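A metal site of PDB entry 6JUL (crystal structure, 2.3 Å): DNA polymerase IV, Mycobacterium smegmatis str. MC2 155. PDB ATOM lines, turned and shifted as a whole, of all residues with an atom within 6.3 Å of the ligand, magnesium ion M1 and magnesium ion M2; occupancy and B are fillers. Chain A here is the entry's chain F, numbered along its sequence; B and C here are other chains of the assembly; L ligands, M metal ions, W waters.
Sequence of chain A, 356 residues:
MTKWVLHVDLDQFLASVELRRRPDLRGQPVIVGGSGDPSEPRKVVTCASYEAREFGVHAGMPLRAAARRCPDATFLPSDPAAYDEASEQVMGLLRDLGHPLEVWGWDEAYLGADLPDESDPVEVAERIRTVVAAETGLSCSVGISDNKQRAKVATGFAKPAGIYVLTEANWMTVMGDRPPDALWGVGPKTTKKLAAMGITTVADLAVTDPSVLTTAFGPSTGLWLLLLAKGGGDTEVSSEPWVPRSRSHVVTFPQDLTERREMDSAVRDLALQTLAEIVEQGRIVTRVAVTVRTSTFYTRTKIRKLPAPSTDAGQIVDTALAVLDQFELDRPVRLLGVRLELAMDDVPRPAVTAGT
NZ of Lys 159 is in salt-bridge range of O3 of the ligand (3.1 Å).
N4 of DC 18 of chain B sits at hydrogen-bond distance from N4 of the ligand.
NH1 of Arg 53 lies within salt-bridge range of O2 of the ligand.
N of Phe 13 sits at hydrogen-bond distance from O5 of the ligand, at 3.5 Å.
O3 of the ligand is in hydrogen-bond range of OH of Tyr 50, 2.7 Å away.
N of Gln 12 lies within hydrogen-bond range of O3 of the ligand (2.8 Å).
An oxygen (O5) of the ligand sits at hydrogen-bond distance from the side-chain sulfur of Cys 47, at 3.4 Å.
O6 of DG 4 of chain C is in hydrogen-bond range of a nitrogen (N4) of the ligand, at 2.9 Å.
The side-chain hydroxyl (OG1) of Thr 46 lies within hydrogen-bond range of an oxygen (O12) of the ligand (2.9 Å).
O8 of the ligand is bound to magnesium ion M1 (2.1 Å).
OD1 of Asp 9 binds magnesium ion M1, at 2.2 Å.
Magnesium ion M1 is bound by an oxygen (O4) of the ligand, 2.2 Å away.
Magnesium ion M1 is bound by O1 of the ligand (2.2 Å).
O of Leu 10 is bound to magnesium ion M1, 2.2 Å away.
Magnesium ion M1 is bound by OD1 of Asp 107.
OD2 of Asp 107 is bound to magnesium ion M1 (2.3 Å).
Merely in contact with magnesium ion M1: Lys 159 (3.98 Å).
Four residues have an atom within 4 Å of magnesium ion M1: Asp 9, Leu 10, Asp 107 and Lys 159.
Four residues have an atom within 4 Å of magnesium ion M2: Asp 9, Asp 107, Glu 108 and DC 18 of chain B.
The side-chain sulfur (SG) of Cys 47 sits at hydrogen-bond distance from the backbone NH (N) of Leu 14, at 3.7 Å.
N of Tyr 50 lies within hydrogen-bond range of OE1 of Gln 12 (2.7 Å).
The backbone carbonyl oxygen (O) of Leu 10 lies close to the side-chain amino group (NZ) of Lys 159 (3.3 Å).
O2 of DC 18 of chain B sits close to N2 of DG 5 of chain C, at 2.7 Å.
NZ of Lys 159 sits at hydrogen-bond distance from O of Asp 9 (3.1 Å).
OE1 of Glu 108 is in salt-bridge range of NZ of Lys 152 (2.9 Å).
The side-chain carboxylate of Asp 11 lies within salt-bridge range of the side-chain amino group of Lys 159 (2.7 Å).
The side-chain sulfur of Cys 47 lies within hydrogen-bond range of the backbone NH of Ala 15 (3.4 Å).
Water W1 lies within hydrogen-bond range of O5 of the ligand (3.0 Å) and O of Thr 46 (3.0 Å).
Residues that only touch the ligand: Asp 11 (3.4 Å), Leu 14 (3.4 Å), Ala 59 (3.7 Å) and DG 5 of chain C (3.96 Å).
Hydrophobic or aromatic side chains that line the ligand: Phe 13, Leu 14, Tyr 50 and Ala 59.
Within 4 Å of the ligand: Asp 9, Leu 10, Asp 11, Gln 12, Phe 13, Leu 14, Thr 46, Cys 47, Tyr 50, Arg 53, Ala 59, Asp 107, Lys 159, DC 18 of chain B, DG 4 of chain C and DG 5 of chain C.
The nearest printed residue that does not touch the ligand is Glu 108 (4.4 Å).
Magnesium ion M2 is bound by the side-chain carboxylate of Glu 108, O3' of DC 18 of chain B, the side-chain carboxylate of Asp 107, the side-chain carboxylate of Asp 9 and an oxygen (O8) of the ligand.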
ATOM      1  N   HIS A   7      17.717  10.092  -4.440  1.00  0.00           N
ATOM      2  CA  HIS A   7      17.364   8.917  -3.655  1.00  0.00           C
ATOM      3  C   HIS A   7      17.790   9.063  -2.203  1.00  0.00           C
ATOM      4  O   HIS A   7      18.998   9.166  -1.911  1.00  0.00           O
ATOM      5  CB  HIS A   7      17.925   7.616  -4.288  1.00  0.00           C
ATOM      6  CG  HIS A   7      17.558   6.394  -3.539  1.00  0.00           C
ATOM      7  ND1 HIS A   7      18.460   5.702  -2.770  1.00  0.00           N
ATOM      8  CD2 HIS A   7      16.343   5.843  -3.307  1.00  0.00           C
ATOM      9  CE1 HIS A   7      17.841   4.714  -2.167  1.00  0.00           C
ATOM     10  NE2 HIS A   7      16.556   4.748  -2.492  1.00  0.00           N
ATOM     11  N   ASP A   9      18.127   7.436   1.486  1.00  0.00           N
ATOM     12  CA  ASP A   9      18.163   6.178   2.150  1.00  0.00           C
ATOM     13  C   ASP A   9      18.648   6.274   3.654  1.00  0.00           C
ATOM     14  O   ASP A   9      19.734   6.667   3.892  1.00  0.00           O
ATOM     15  CB  ASP A   9      18.921   5.160   1.323  1.00  0.00           C
ATOM     16  CG  ASP A   9      18.916   3.747   1.941  1.00  0.00           C
ATOM     17  OD1 ASP A   9      19.547   3.582   3.031  1.00  0.00           O
ATOM     18  OD2 ASP A   9      18.281   2.817   1.376  1.00  0.00           O
ATOM     19  N   LEU A  10      17.804   5.918   4.619  1.00  0.00           N
ATOM     20  CA  LEU A  10      18.209   5.889   6.038  1.00  0.00           C
ATOM     21  C   LEU A  10      19.376   4.928   6.370  1.00  0.00           C
ATOM     22  O   LEU A  10      19.429   3.743   5.860  1.00  0.00           O
ATOM     23  CB  LEU A  10      16.976   5.560   6.885  1.00  0.00           C
ATOM     24  CG  LEU A  10      16.105   6.828   6.825  1.00  0.00           C
ATOM     25  CD1 LEU A  10      14.699   6.440   7.157  1.00  0.00           C
ATOM     26  CD2 LEU A  10      16.675   7.875   7.825  1.00  0.00           C
ATOM     27  N   ASP A  11      20.349   5.456   7.094  1.00  0.00           N
ATOM     28  CA  ASP A  11      21.568   4.731   7.482  1.00  0.00           C
ATOM     29  C   ASP A  11      21.267   3.720   8.533  1.00  0.00           C
ATOM     30  O   ASP A  11      20.673   4.068   9.572  1.00  0.00           O
ATOM     31  CB  ASP A  11      22.701   5.646   7.936  1.00  0.00           C
ATOM     32  CG  ASP A  11      23.239   6.507   6.831  1.00  0.00           C
ATOM     33  OD1 ASP A  11      22.959   6.294   5.589  1.00  0.00           O
ATOM     34  OD2 ASP A  11      23.921   7.454   7.150  1.00  0.00           O
ATOM     35  N   GLN A  12      21.629   2.461   8.256  1.00  0.00           N
ATOM     36  CA  GLN A  12      21.489   1.308   9.201  1.00  0.00           C
ATOM     37  C   GLN A  12      20.140   1.425   9.988  1.00  0.00           C
ATOM     38  O   GLN A  12      20.113   1.472  11.208  1.00  0.00           O
ATOM     39  CB  GLN A  12      22.747   1.179  10.099  1.00  0.00           C
ATOM     40  CG  GLN A  12      22.895   2.314  11.154  1.00  0.00           C
ATOM     41  CD  GLN A  12      24.058   2.226  12.124  1.00  0.00           C
ATOM     42  OE1 GLN A  12      24.481   1.159  12.488  1.00  0.00           O
ATOM     43  NE2 GLN A  12      24.602   3.341  12.512  1.00  0.00           N
ATOM     44  N   PHE A  13      19.050   1.566   9.221  1.00  0.00           N
ATOM     45  CA  PHE A  13      17.800   2.072   9.705  1.00  0.00           C
ATOM     46  C   PHE A  13      17.349   1.425  11.054  1.00  0.00           C
ATOM     47  O   PHE A  13      17.133   2.166  12.026  1.00  0.00           O
ATOM     48  CB  PHE A  13      16.743   1.920   8.662  1.00  0.00           C
ATOM     49  CG  PHE A  13      15.376   2.372   9.123  1.00  0.00           C
ATOM     50  CD1 PHE A  13      15.199   3.637   9.747  1.00  0.00           C
ATOM     51  CD2 PHE A  13      14.234   1.557   8.942  1.00  0.00           C
ATOM     52  CE1 PHE A  13      13.939   4.033  10.190  1.00  0.00           C
ATOM     53  CE2 PHE A  13      12.977   1.977   9.423  1.00  0.00           C
ATOM     54  CZ  PHE A  13      12.830   3.220  10.021  1.00  0.00           C
ATOM     55  N   LEU A  14      17.216   0.110  11.157  1.00  0.00           N
ATOM     56  CA  LEU A  14      16.566  -0.412  12.389  1.00  0.00           C
ATOM     57  C   LEU A  14      17.499  -0.206  13.565  1.00  0.00           C
ATOM     58  O   LEU A  14      17.110   0.254  14.608  1.00  0.00           O
ATOM     59  CB  LEU A  14      16.165  -1.860  12.245  1.00  0.00           C
ATOM     60  CG  LEU A  14      14.910  -2.337  11.464  1.00  0.00           C
ATOM     61  CD1 LEU A  14      14.507  -1.663  10.225  1.00  0.00           C
ATOM     62  CD2 LEU A  14      15.097  -3.820  11.131  1.00  0.00           C
ATOM     63  N   ALA A  15      18.766  -0.489  13.365  1.00  0.00           N
ATOM     64  CA  ALA A  15      19.754  -0.211  14.406  1.00  0.00           C
ATOM     65  C   ALA A  15      19.735   1.255  14.874  1.00  0.00           C
ATOM     66  O   ALA A  15      19.863   1.528  16.122  1.00  0.00           O
ATOM     67  CB  ALA A  15      21.141  -0.610  13.969  1.00  0.00           C
ATOM     68  N   VAL A  45      19.465 -12.124  10.954  1.00  0.00           N
ATOM     69  CA  VAL A  45      19.703 -10.721  11.115  1.00  0.00           C
ATOM     70  C   VAL A  45      18.911  -9.925  10.096  1.00  0.00           C
ATOM     71  O   VAL A  45      18.898 -10.194   8.871  1.00  0.00           O
ATOM     72  CB  VAL A  45      21.180 -10.358  10.989  1.00  0.00           C
ATOM     73  CG1 VAL A  45      21.370  -8.819  11.037  1.00  0.00           C
ATOM     74  CG2 VAL A  45      22.052 -11.061  12.062  1.00  0.00           C
ATOM     75  N   THR A  46      18.254  -8.915  10.633  1.00  0.00           N
ATOM     76  CA  THR A  46      17.542  -8.013   9.789  1.00  0.00           C
ATOM     77  C   THR A  46      18.211  -6.610   9.588  1.00  0.00           C
ATOM     78  O   THR A  46      18.110  -6.043   8.540  1.00  0.00           O
ATOM     79  CB  THR A  46      16.108  -8.026  10.242  1.00  0.00           C
ATOM     80  OG1 THR A  46      15.395  -7.689   9.110  1.00  0.00           O
ATOM     81  CG2 THR A  46      15.862  -7.022  11.290  1.00  0.00           C
ATOM     82  N   CYS A  47      18.965  -6.115  10.577  1.00  0.00           N
ATOM     83  CA  CYS A  47      19.742  -4.962  10.479  1.00  0.00           C
ATOM     84  C   CYS A  47      20.869  -5.040  11.482  1.00  0.00           C
ATOM     85  O   CYS A  47      20.647  -5.027  12.707  1.00  0.00           O
ATOM     86  CB  CYS A  47      18.898  -3.702  10.734  1.00  0.00           C
ATOM     87  SG  CYS A  47      19.991  -2.226  10.727  1.00  0.00           S
ATOM     88  N   ALA A  48      22.072  -5.087  10.984  1.00  0.00           N
ATOM     89  CA  ALA A  48      23.248  -5.057  11.859  1.00  0.00           C
ATOM     90  C   ALA A  48      23.689  -3.607  11.887  1.00  0.00           C
ATOM     91  O   ALA A  48      23.642  -2.912  10.818  1.00  0.00           O
ATOM     92  CB  ALA A  48      24.322  -5.929  11.259  1.00  0.00           C
ATOM     93  N   TYR A  50      26.450  -0.616  11.902  1.00  0.00           N
ATOM     94  CA  TYR A  50      27.788  -0.558  11.293  1.00  0.00           C
ATOM     95  C   TYR A  50      28.871  -1.288  12.059  1.00  0.00           C
ATOM     96  O   TYR A  50      29.768  -1.885  11.413  1.00  0.00           O
ATOM     97  CB  TYR A  50      28.216   0.843  10.925  1.00  0.00           C
ATOM     98  CG  TYR A  50      27.291   1.530   9.918  1.00  0.00           C
ATOM     99  CD1 TYR A  50      26.539   0.796   9.019  1.00  0.00           C
ATOM    100  CD2 TYR A  50      27.223   2.909   9.856  1.00  0.00           C
ATOM    101  CE1 TYR A  50      25.712   1.383   8.052  1.00  0.00           C
ATOM    102  CE2 TYR A  50      26.425   3.580   8.874  1.00  0.00           C
ATOM    103  CZ  TYR A  50      25.646   2.810   7.973  1.00  0.00           C
ATOM    104  OH  TYR A  50      24.866   3.424   6.985  1.00  0.00           O
ATOM    105  N   ARG A  53      28.790  -4.830  11.364  1.00  0.00           N
ATOM    106  CA  ARG A  53      29.117  -5.219   9.935  1.00  0.00           C
ATOM    107  C   ARG A  53      30.635  -5.354   9.869  1.00  0.00           C
ATOM    108  O   ARG A  53      31.165  -6.078   9.046  1.00  0.00           O
ATOM    109  CB  ARG A  53      28.585  -4.186   8.884  1.00  0.00           C
ATOM    110  CG  ARG A  53      27.024  -4.181   8.744  1.00  0.00           C
ATOM    111  CD  ARG A  53      26.427  -3.121   7.824  1.00  0.00           C
ATOM    112  NE  ARG A  53      25.055  -2.669   8.226  1.00  0.00           N
ATOM    113  CZ  ARG A  53      24.149  -2.043   7.441  1.00  0.00           C
ATOM    114  NH1 ARG A  53      24.444  -1.640   6.235  1.00  0.00           N
ATOM    115  NH2 ARG A  53      22.964  -1.682   7.940  1.00  0.00           N
ATOM    116  N   ALA A  59      22.414  -8.231   6.846  1.00  0.00           N
ATOM    117  CA  ALA A  59      21.013  -8.630   6.685  1.00  0.00           C
ATOM    118  C   ALA A  59      20.963  -9.978   6.007  1.00  0.00           C
ATOM    119  O   ALA A  59      21.515 -10.095   4.943  1.00  0.00           O
ATOM    120  CB  ALA A  59      20.249  -7.571   5.858  1.00  0.00           C
ATOM    121  N   GLY A  60      20.258 -10.977   6.594  1.00  0.00           N
ATOM    122  CA  GLY A  60      19.945 -12.272   5.939  1.00  0.00           C
ATOM    123  C   GLY A  60      20.811 -13.342   6.581  1.00  0.00           C
ATOM    124  O   GLY A  60      20.532 -14.561   6.488  1.00  0.00           O
ATOM    125  N   TRP A 106      10.032   1.110   4.359  1.00  0.00           N
ATOM    126  CA  TRP A 106      10.279   1.865   5.565  1.00  0.00           C
ATOM    127  C   TRP A 106      11.301   2.962   5.280  1.00  0.00           C
ATOM    128  O   TRP A 106      11.141   4.027   5.822  1.00  0.00           O
ATOM    129  CB  TRP A 106      10.885   0.972   6.641  1.00  0.00           C
ATOM    130  CG  TRP A 106       9.981   0.201   7.535  1.00  0.00           C
ATOM    131  CD1 TRP A 106       8.722   0.575   8.051  1.00  0.00           C
ATOM    132  CD2 TRP A 106      10.299  -1.031   8.179  1.00  0.00           C
ATOM    133  NE1 TRP A 106       8.239  -0.388   8.912  1.00  0.00           N
ATOM    134  CE2 TRP A 106       9.177  -1.396   8.995  1.00  0.00           C
ATOM    135  CE3 TRP A 106      11.385  -1.921   8.063  1.00  0.00           C
ATOM    136  CZ2 TRP A 106       9.155  -2.546   9.741  1.00  0.00           C
ATOM    137  CZ3 TRP A 106      11.359  -3.083   8.770  1.00  0.00           C
ATOM    138  CH2 TRP A 106      10.256  -3.396   9.609  1.00  0.00           C
ATOM    139  N   ASP A 107      12.299   2.679   4.425  1.00  0.00           N
ATOM    140  CA  ASP A 107      13.673   3.192   4.591  1.00  0.00           C
ATOM    141  C   ASP A 107      14.028   4.181   3.530  1.00  0.00           C
ATOM    142  O   ASP A 107      15.049   4.917   3.668  1.00  0.00           O
ATOM    143  CB  ASP A 107      14.667   1.975   4.371  1.00  0.00           C
ATOM    144  CG  ASP A 107      16.165   2.386   4.357  1.00  0.00           C
ATOM    145  OD1 ASP A 107      16.784   2.680   5.362  1.00  0.00           O
ATOM    146  OD2 ASP A 107      16.851   2.460   3.313  1.00  0.00           O
ATOM    147  N   GLU A 108      13.288   4.113   2.408  1.00  0.00           N
ATOM    148  CA  GLU A 108      13.680   4.862   1.228  1.00  0.00           C
ATOM    149  C   GLU A 108      12.588   5.600   0.396  1.00  0.00           C
ATOM    150  O   GLU A 108      11.399   5.317   0.472  1.00  0.00           O
ATOM    151  CB  GLU A 108      14.487   3.995   0.268  1.00  0.00           C
ATOM    152  CG  GLU A 108      14.222   2.546   0.281  1.00  0.00           C
ATOM    153  CD  GLU A 108      15.157   1.955  -0.709  1.00  0.00           C
ATOM    154  OE1 GLU A 108      15.062   2.387  -1.894  1.00  0.00           O
ATOM    155  OE2 GLU A 108      16.064   1.160  -0.307  1.00  0.00           O
ATOM    156  N   LYS A 152      20.118   5.324  -7.148  1.00  0.00           N
ATOM    157  CA  LYS A 152      20.132   4.242  -6.235  1.00  0.00           C
ATOM    158  C   LYS A 152      21.580   3.799  -6.169  1.00  0.00           C
ATOM    159  O   LYS A 152      22.139   3.724  -5.083  1.00  0.00           O
ATOM    160  CB  LYS A 152      19.083   3.195  -6.734  1.00  0.00           C
ATOM    161  CG  LYS A 152      18.907   2.011  -5.873  1.00  0.00           C
ATOM    162  CD  LYS A 152      18.112   2.423  -4.655  1.00  0.00           C
ATOM    163  CE  LYS A 152      17.198   1.301  -4.112  1.00  0.00           C
ATOM    164  NZ  LYS A 152      17.485   1.074  -2.654  1.00  0.00           N
ATOM    165  N   LYS A 159      27.047   6.328   0.937  1.00  0.00           N
ATOM    166  CA  LYS A 159      27.099   5.640   2.255  1.00  0.00           C
ATOM    167  C   LYS A 159      28.518   5.735   2.896  1.00  0.00           C
ATOM    168  O   LYS A 159      29.528   5.491   2.193  1.00  0.00           O
ATOM    169  CB  LYS A 159      26.733   4.125   2.147  1.00  0.00           C
ATOM    170  CG  LYS A 159      25.228   3.813   1.954  1.00  0.00           C
ATOM    171  CD  LYS A 159      24.390   4.173   3.166  1.00  0.00           C
ATOM    172  CE  LYS A 159      22.918   4.135   2.739  1.00  0.00           C
ATOM    173  NZ  LYS A 159      21.924   4.493   3.836  1.00  0.00           N
ATOM    174  P    DC B  18      17.872  -2.570  -2.493  1.00  0.00           P
ATOM    175  OP1  DC B  18      18.243  -1.215  -2.867  1.00  0.00           O
ATOM    176  OP2  DC B  18      18.886  -3.572  -2.114  1.00  0.00           O
ATOM    177  O5'  DC B  18      16.802  -2.596  -1.319  1.00  0.00           O
ATOM    178  C5'  DC B  18      15.527  -1.884  -1.421  1.00  0.00           C
ATOM    179  C4'  DC B  18      14.735  -2.113  -0.151  1.00  0.00           C
ATOM    180  O4'  DC B  18      14.281  -3.483  -0.152  1.00  0.00           O
ATOM    181  C3'  DC B  18      15.592  -1.949   1.112  1.00  0.00           C
ATOM    182  O3'  DC B  18      15.496  -0.642   1.708  1.00  0.00           O
ATOM    183  C2'  DC B  18      15.071  -3.021   2.031  1.00  0.00           C
ATOM    184  C1'  DC B  18      14.304  -4.003   1.147  1.00  0.00           C
ATOM    185  N1   DC B  18      14.805  -5.387   1.075  1.00  0.00           N
ATOM    186  C2   DC B  18      14.047  -6.361   1.706  1.00  0.00           C
ATOM    187  O2   DC B  18      13.034  -6.013   2.310  1.00  0.00           O
ATOM    188  N3   DC B  18      14.391  -7.668   1.579  1.00  0.00           N
ATOM    189  C4   DC B  18      15.514  -7.998   0.920  1.00  0.00           C
ATOM    190  N4   DC B  18      15.858  -9.298   0.863  1.00  0.00           N
ATOM    191  C5   DC B  18      16.333  -7.015   0.288  1.00  0.00           C
ATOM    192  C6   DC B  18      15.948  -5.725   0.394  1.00  0.00           C
ATOM    193  P    DG C   4      15.443 -18.952   5.808  1.00  0.00           P
ATOM    194  OP1  DG C   4      14.825 -20.188   6.292  1.00  0.00           O
ATOM    195  OP2  DG C   4      15.257 -18.500   4.441  1.00  0.00           O
ATOM    196  O5'  DG C   4      14.987 -17.714   6.697  1.00  0.00           O
ATOM    197  C5'  DG C   4      14.861 -17.756   8.113  1.00  0.00           C
ATOM    198  C4'  DG C   4      13.771 -16.785   8.511  1.00  0.00           C
ATOM    199  O4'  DG C   4      14.212 -15.440   8.218  1.00  0.00           O
ATOM    200  C3'  DG C   4      12.464 -16.969   7.757  1.00  0.00           C
ATOM    201  O3'  DG C   4      11.358 -16.748   8.654  1.00  0.00           O
ATOM    202  C2'  DG C   4      12.586 -15.959   6.608  1.00  0.00           C
ATOM    203  C1'  DG C   4      13.417 -14.841   7.227  1.00  0.00           C
ATOM    204  N9   DG C   4      14.348 -14.168   6.344  1.00  0.00           N
ATOM    205  C8   DG C   4      15.338 -14.791   5.624  1.00  0.00           C
ATOM    206  N7   DG C   4      16.079 -13.972   4.946  1.00  0.00           N
ATOM    207  C5   DG C   4      15.574 -12.719   5.265  1.00  0.00           C
ATOM    208  C6   DG C   4      16.012 -11.437   4.851  1.00  0.00           C
ATOM    209  O6   DG C   4      16.932 -11.143   4.085  1.00  0.00           O
ATOM    210  N1   DG C   4      15.220 -10.437   5.390  1.00  0.00           N
ATOM    211  C2   DG C   4      14.160 -10.626   6.245  1.00  0.00           C
ATOM    212  N2   DG C   4      13.556  -9.498   6.676  1.00  0.00           N
ATOM    213  N3   DG C   4      13.790 -11.824   6.695  1.00  0.00           N
ATOM    214  C4   DG C   4      14.528 -12.818   6.150  1.00  0.00           C
ATOM    215  P    DG C   5       9.854 -16.846   8.083  1.00  0.00           P
ATOM    216  OP1  DG C   5       8.972 -17.307   9.141  1.00  0.00           O
ATOM    217  OP2  DG C   5       9.849 -17.667   6.808  1.00  0.00           O
ATOM    218  O5'  DG C   5       9.604 -15.317   7.669  1.00  0.00           O
ATOM    219  C5'  DG C   5       9.450 -14.233   8.580  1.00  0.00           C
ATOM    220  C4'  DG C   5       8.952 -13.052   7.774  1.00  0.00           C
ATOM    221  O4'  DG C   5      10.039 -12.559   6.967  1.00  0.00           O
ATOM    222  C3'  DG C   5       7.785 -13.324   6.826  1.00  0.00           C
ATOM    223  O3'  DG C   5       6.843 -12.279   7.029  1.00  0.00           O
ATOM    224  C2'  DG C   5       8.405 -13.290   5.432  1.00  0.00           C
ATOM    225  C1'  DG C   5       9.535 -12.300   5.652  1.00  0.00           C
ATOM    226  N9   DG C   5      10.654 -12.369   4.709  1.00  0.00           N
ATOM    227  C8   DG C   5      11.258 -13.501   4.243  1.00  0.00           C
ATOM    228  N7   DG C   5      12.243 -13.254   3.417  1.00  0.00           N
ATOM    229  C5   DG C   5      12.301 -11.864   3.360  1.00  0.00           C
ATOM    230  C6   DG C   5      13.208 -10.995   2.652  1.00  0.00           C
ATOM    231  O6   DG C   5      14.125 -11.297   1.892  1.00  0.00           O
ATOM    232  N1   DG C   5      12.905  -9.660   2.886  1.00  0.00           N
ATOM    233  C2   DG C   5      11.894  -9.198   3.693  1.00  0.00           C
ATOM    234  N2   DG C   5      11.795  -7.871   3.817  1.00  0.00           N
ATOM    235  N3   DG C   5      11.104  -9.987   4.403  1.00  0.00           N
ATOM    236  C4   DG C   5      11.350 -11.308   4.173  1.00  0.00           C
HETATM  237  P1  LIG L   1      22.160   0.932   5.058  1.00  0.00           P
HETATM  238  O1  LIG L   1      20.897   1.509   4.291  1.00  0.00           O
HETATM  239  O2  LIG L   1      23.186   0.041   4.425  1.00  0.00           O
HETATM  240  O3  LIG L   1      22.806   2.145   5.737  1.00  0.00           O
HETATM  241  P2  LIG L   1      19.946  -0.530   6.234  1.00  0.00           P
HETATM  242  O4  LIG L   1      19.083   0.750   6.151  1.00  0.00           O
HETATM  243  O5  LIG L   1      19.646  -1.357   7.463  1.00  0.00           O
HETATM  244  O6  LIG L   1      21.453  -0.001   6.189  1.00  0.00           O
HETATM  245  P3  LIG L   1      18.640  -1.186   3.615  1.00  0.00           P
HETATM  246  O7  LIG L   1      19.244  -2.007   2.541  1.00  0.00           O
HETATM  247  O8  LIG L   1      18.330   0.314   3.413  1.00  0.00           O
HETATM  248  N1  LIG L   1      19.773  -1.334   4.824  1.00  0.00           N
HETATM  249  O9  LIG L   1      17.328  -1.914   4.140  1.00  0.00           O
HETATM  250  C1  LIG L   1      16.523  -1.135   5.074  1.00  0.00           C
HETATM  251  C2  LIG L   1      15.735  -1.934   6.081  1.00  0.00           C
HETATM  252  O10 LIG L   1      15.060  -2.940   5.344  1.00  0.00           O
HETATM  253  C3  LIG L   1      16.643  -2.640   7.049  1.00  0.00           C
HETATM  254  O11 LIG L   1      17.186  -1.857   8.118  1.00  0.00           O
HETATM  255  C4  LIG L   1      15.823  -3.823   7.470  1.00  0.00           C
HETATM  256  C5  LIG L   1      15.038  -4.111   6.163  1.00  0.00           C
HETATM  257  N2  LIG L   1      15.741  -5.193   5.418  1.00  0.00           N
HETATM  258  C6  LIG L   1      15.397  -6.514   5.638  1.00  0.00           C
HETATM  259  N3  LIG L   1      16.019  -7.471   4.944  1.00  0.00           N
HETATM  260  C7  LIG L   1      17.018  -7.267   4.053  1.00  0.00           C
HETATM  261  C8  LIG L   1      17.435  -5.965   3.766  1.00  0.00           C
HETATM  262  C9  LIG L   1      16.775  -4.954   4.506  1.00  0.00           C
HETATM  263  O12 LIG L   1      14.547  -6.822   6.470  1.00  0.00           O
HETATM  264  N4  LIG L   1      17.574  -8.349   3.466  1.00  0.00           N
HETATM  265 MG    MG M   1      18.789   2.126   4.475  1.00  0.00          MG
HETATM  266 MG    MG M   2      17.031   0.963   1.674  1.00  0.00          MG
HETATM  267  O   HOH W   1      20.029  -4.282   7.047  1.00  0.00           O
HETATM  268  O   HOH W   2      20.879   1.046   1.536  1.00  0.00           O
